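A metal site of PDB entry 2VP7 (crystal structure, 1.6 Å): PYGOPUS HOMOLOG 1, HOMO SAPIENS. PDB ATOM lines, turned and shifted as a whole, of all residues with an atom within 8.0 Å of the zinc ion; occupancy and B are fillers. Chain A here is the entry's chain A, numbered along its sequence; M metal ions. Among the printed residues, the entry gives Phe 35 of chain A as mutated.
The backbone carbonyl oxygen (O) of Cys 28 lies within hydrogen-bond range of the backbone NH (N) of Gln 33 (3.0 Å). The backbone NH (N) of Ala 30 lies close to the side-chain sulfur (SG) of Cys 28, 3.6 Å away. N of Lys 34 sits close to SG of Cys 32, at 3.4 Å. N of Cys 28 lies within hydrogen-bond range of O of Lys 34 (2.9 Å).
Within 4 Å of the zinc ion: Cys 28, Cys 32, Cys 61 and Cys 64. The nearest printed residue that does not touch the zinc ion is Gln 33 (4.7 Å).
The zinc ion is bound by SG of Cys 61 (2.1 Å), SG of Cys 32 (2.2 Å), SG of Cys 28 (2.2 Å) and SG of Cys 64 (2.6 Å). The zinc ion has four donor atoms within binding distance.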
ATOM      1  N   LEU A  27     -18.111  27.416   2.319  1.00  0.00           N
ATOM      2  CA  LEU A  27     -18.526  26.192   2.995  1.00  0.00           C
ATOM      3  C   LEU A  27     -19.814  26.453   3.740  1.00  0.00           C
ATOM      4  O   LEU A  27     -19.891  27.413   4.523  1.00  0.00           O
ATOM      5  CB  LEU A  27     -17.447  25.774   4.003  1.00  0.00           C
ATOM      6  CG  LEU A  27     -17.764  24.596   4.941  1.00  0.00           C
ATOM      7  CD1 LEU A  27     -17.846  23.310   4.146  1.00  0.00           C
ATOM      8  CD2 LEU A  27     -16.699  24.536   6.005  1.00  0.00           C
ATOM      9  N   CYS A  28     -20.818  25.613   3.531  1.00  0.00           N
ATOM     10  CA  CYS A  28     -22.017  25.736   4.342  1.00  0.00           C
ATOM     11  C   CYS A  28     -21.710  25.231   5.752  1.00  0.00           C
ATOM     12  O   CYS A  28     -21.422  24.051   5.966  1.00  0.00           O
ATOM     13  CB  CYS A  28     -23.201  25.031   3.731  1.00  0.00           C
ATOM     14  SG  CYS A  28     -24.655  25.123   4.791  1.00  0.00           S
ATOM     15  N   GLU A  29     -21.739  26.150   6.711  1.00  0.00           N
ATOM     16  CA  GLU A  29     -21.453  25.803   8.097  1.00  0.00           C
ATOM     17  C   GLU A  29     -22.744  25.756   8.907  1.00  0.00           C
ATOM     18  O   GLU A  29     -22.701  25.565  10.129  1.00  0.00           O
ATOM     19  CB  GLU A  29     -20.469  26.797   8.718  1.00  0.00           C
ATOM     20  CG  GLU A  29     -19.071  26.759   8.122  1.00  0.00           C
ATOM     21  CD  GLU A  29     -18.093  27.656   8.849  1.00  0.00           C
ATOM     22  OE1 GLU A  29     -17.765  27.348  10.028  1.00  0.00           O
ATOM     23  OE2 GLU A  29     -17.653  28.660   8.274  1.00  0.00           O
ATOM     24  N   ALA A  30     -23.880  25.921   8.237  1.00  0.00           N
ATOM     25  CA  ALA A  30     -25.172  25.807   8.930  1.00  0.00           C
ATOM     26  C   ALA A  30     -25.341  24.369   9.409  1.00  0.00           C
ATOM     27  O   ALA A  30     -25.567  24.110  10.609  1.00  0.00           O
ATOM     28  CB  ALA A  30     -26.309  26.208   8.026  1.00  0.00           C
ATOM     29  N   SER A  31     -25.230  23.428   8.473  1.00  0.00           N
ATOM     30  CA  SER A  31     -25.252  22.021   8.826  1.00  0.00           C
ATOM     31  C   SER A  31     -24.553  21.133   7.800  1.00  0.00           C
ATOM     32  O   SER A  31     -23.645  20.375   8.166  1.00  0.00           O
ATOM     33  CB  SER A  31     -26.689  21.535   9.057  1.00  0.00           C
ATOM     34  OG  SER A  31     -26.671  20.217   9.567  1.00  0.00           O
ATOM     35  N   CYS A  32     -24.952  21.264   6.531  1.00  0.00           N
ATOM     36  CA  CYS A  32     -24.538  20.313   5.481  1.00  0.00           C
ATOM     37  C   CYS A  32     -23.029  20.149   5.237  1.00  0.00           C
ATOM     38  O   CYS A  32     -22.570  19.048   4.909  1.00  0.00           O
ATOM     39  CB  CYS A  32     -25.306  20.532   4.164  1.00  0.00           C
ATOM     40  SG  CYS A  32     -24.741  21.885   3.090  1.00  0.00           S
ATOM     41  N   GLN A  33     -22.262  21.225   5.400  1.00  0.00           N
ATOM     42  CA  GLN A  33     -20.822  21.176   5.184  1.00  0.00           C
ATOM     43  C   GLN A  33     -20.475  20.891   3.710  1.00  0.00           C
ATOM     44  O   GLN A  33     -19.434  20.309   3.432  1.00  0.00           O
ATOM     45  CB  GLN A  33     -20.190  20.100   6.058  1.00  0.00           C
ATOM     46  CG  GLN A  33     -18.929  20.528   6.791  1.00  0.00           C
ATOM     47  CD  GLN A  33     -19.226  20.931   8.218  1.00  0.00           C
ATOM     48  OE1 GLN A  33     -20.382  21.155   8.573  1.00  0.00           O
ATOM     49  NE2 GLN A  33     -18.191  20.996   9.056  1.00  0.00           N
ATOM     50  N   LYS A  34     -21.380  21.268   2.811  1.00  0.00           N
ATOM     51  CA  LYS A  34     -21.128  21.227   1.358  1.00  0.00           C
ATOM     52  C   LYS A  34     -20.329  22.476   0.967  1.00  0.00           C
ATOM     53  O   LYS A  34     -20.470  23.543   1.595  1.00  0.00           O
ATOM     54  CB  LYS A  34     -22.443  21.179   0.571  1.00  0.00           C
ATOM     55  CG  LYS A  34     -23.280  19.878   0.741  1.00  0.00           C
ATOM     56  CD  LYS A  34     -24.346  19.714  -0.364  1.00  0.00           C
ATOM     57  CE  LYS A  34     -25.523  20.668  -0.235  1.00  0.00           C
ATOM     58  NZ  LYS A  34     -26.590  20.421  -1.276  1.00  0.00           N
ATOM     59  N   PHE A  35     -19.461  22.324  -0.040  1.00  0.00           N
ATOM     60  CA  PHE A  35     -18.748  23.463  -0.623  1.00  0.00           C
ATOM     61  C   PHE A  35     -19.437  23.953  -1.857  1.00  0.00           C
ATOM     62  O   PHE A  35     -20.173  23.208  -2.502  1.00  0.00           O
ATOM     63  CB  PHE A  35     -17.331  23.085  -0.990  1.00  0.00           C
ATOM     64  CG  PHE A  35     -16.412  23.069   0.166  1.00  0.00           C
ATOM     65  CD1 PHE A  35     -15.839  24.249   0.618  1.00  0.00           C
ATOM     66  CD2 PHE A  35     -16.154  21.874   0.834  1.00  0.00           C
ATOM     67  CE1 PHE A  35     -14.982  24.256   1.699  1.00  0.00           C
ATOM     68  CE2 PHE A  35     -15.312  21.856   1.922  1.00  0.00           C
ATOM     69  CZ  PHE A  35     -14.715  23.043   2.352  1.00  0.00           C
ATOM     70  N   PHE A  36     -19.207  25.225  -2.179  1.00  0.00           N
ATOM     71  CA  PHE A  36     -19.876  25.858  -3.318  1.00  0.00           C
ATOM     72  C   PHE A  36     -18.911  26.884  -3.877  1.00  0.00           C
ATOM     73  O   PHE A  36     -18.174  27.522  -3.147  1.00  0.00           O
ATOM     74  CB  PHE A  36     -21.113  26.629  -2.873  1.00  0.00           C
ATOM     75  CG  PHE A  36     -22.211  25.793  -2.241  1.00  0.00           C
ATOM     76  CD1 PHE A  36     -23.376  25.503  -2.947  1.00  0.00           C
ATOM     77  CD2 PHE A  36     -22.105  25.368  -0.921  1.00  0.00           C
ATOM     78  CE1 PHE A  36     -24.411  24.764  -2.344  1.00  0.00           C
ATOM     79  CE2 PHE A  36     -23.122  24.608  -0.323  1.00  0.00           C
ATOM     80  CZ  PHE A  36     -24.259  24.324  -1.034  1.00  0.00           C
ATOM     81  N   TRP A  59     -21.641  31.079   6.838  1.00  0.00           N
ATOM     82  CA  TRP A  59     -22.625  31.103   5.773  1.00  0.00           C
ATOM     83  C   TRP A  59     -23.455  29.831   5.778  1.00  0.00           C
ATOM     84  O   TRP A  59     -22.949  28.759   6.135  1.00  0.00           O
ATOM     85  CB  TRP A  59     -21.933  31.257   4.413  1.00  0.00           C
ATOM     86  CG  TRP A  59     -22.826  31.204   3.205  1.00  0.00           C
ATOM     87  CD1 TRP A  59     -23.613  32.204   2.722  1.00  0.00           C
ATOM     88  CD2 TRP A  59     -22.988  30.098   2.287  1.00  0.00           C
ATOM     89  NE1 TRP A  59     -24.275  31.798   1.564  1.00  0.00           N
ATOM     90  CE2 TRP A  59     -23.910  30.505   1.281  1.00  0.00           C
ATOM     91  CE3 TRP A  59     -22.453  28.795   2.235  1.00  0.00           C
ATOM     92  CZ2 TRP A  59     -24.289  29.665   0.215  1.00  0.00           C
ATOM     93  CZ3 TRP A  59     -22.846  27.953   1.171  1.00  0.00           C
ATOM     94  CH2 TRP A  59     -23.740  28.409   0.176  1.00  0.00           C
ATOM     95  N   GLY A  60     -24.701  29.973   5.360  1.00  0.00           N
ATOM     96  CA  GLY A  60     -25.646  28.863   5.230  1.00  0.00           C
ATOM     97  C   GLY A  60     -26.249  28.813   3.852  1.00  0.00           C
ATOM     98  O   GLY A  60     -26.709  29.831   3.335  1.00  0.00           O
ATOM     99  N   CYS A  61     -26.223  27.614   3.261  1.00  0.00           N
ATOM    100  CA  CYS A  61     -26.872  27.279   1.970  1.00  0.00           C
ATOM    101  C   CYS A  61     -28.371  27.622   1.937  1.00  0.00           C
ATOM    102  O   CYS A  61     -29.025  27.615   2.989  1.00  0.00           O
ATOM    103  CB  CYS A  61     -26.615  25.770   1.591  1.00  0.00           C
ATOM    104  SG  CYS A  61     -27.521  24.241   2.382  1.00  0.00           S
ATOM    105  N   ASP A  62     -28.909  27.952   0.760  1.00  0.00           N
ATOM    106  CA  ASP A  62     -30.340  28.309   0.632  1.00  0.00           C
ATOM    107  C   ASP A  62     -31.277  27.155   1.010  1.00  0.00           C
ATOM    108  O   ASP A  62     -32.413  27.371   1.426  1.00  0.00           O
ATOM    109  CB  ASP A  62     -30.676  28.817  -0.778  1.00  0.00           C
ATOM    110  CG  ASP A  62     -30.389  30.301  -0.965  1.00  0.00           C
ATOM    111  OD1 ASP A  62     -30.365  31.057   0.036  1.00  0.00           O
ATOM    112  OD2 ASP A  62     -30.201  30.708  -2.133  1.00  0.00           O
ATOM    113  N   THR A  63     -30.773  25.923   0.870  1.00  0.00           N
ATOM    114  CA  THR A  63     -31.512  24.742   1.307  1.00  0.00           C
ATOM    115  C   THR A  63     -31.546  24.711   2.835  1.00  0.00           C
ATOM    116  O   THR A  63     -32.638  24.685   3.430  1.00  0.00           O
ATOM    117  CB  THR A  63     -30.879  23.438   0.757  1.00  0.00           C
ATOM    118  OG1 THR A  63     -30.764  23.529  -0.664  1.00  0.00           O
ATOM    119  CG2 THR A  63     -31.719  22.219   1.117  1.00  0.00           C
ATOM    120  N   CYS A  64     -30.371  24.728   3.469  1.00  0.00           N
ATOM    121  CA  CYS A  64     -30.265  24.663   4.926  1.00  0.00           C
ATOM    122  C   CYS A  64     -31.011  25.796   5.632  1.00  0.00           C
ATOM    123  O   CYS A  64     -31.578  25.592   6.710  1.00  0.00           O
ATOM    124  CB  CYS A  64     -28.801  24.637   5.375  1.00  0.00           C
ATOM    125  SG  CYS A  64     -27.982  23.030   5.242  1.00  0.00           S
ATOM    126  N   MET A  65     -31.022  26.977   5.020  1.00  0.00           N
ATOM    127  CA  MET A  65     -31.691  28.128   5.613  1.00  0.00           C
ATOM    128  C   MET A  65     -33.217  28.000   5.618  1.00  0.00           C
ATOM    129  O   MET A  65     -33.884  28.472   6.539  1.00  0.00           O
ATOM    130  CB  MET A  65     -31.224  29.431   4.944  1.00  0.00           C
ATOM    131  CG  MET A  65     -29.742  29.754   5.182  1.00  0.00           C
ATOM    132  SD  MET A  65     -29.259  29.799   6.931  1.00  0.00           S
ATOM    133  CE  MET A  65     -29.806  31.449   7.397  1.00  0.00           C
HETATM  134 ZN    ZN M   1     -25.975  23.637   3.743  1.00  0.00          ZN
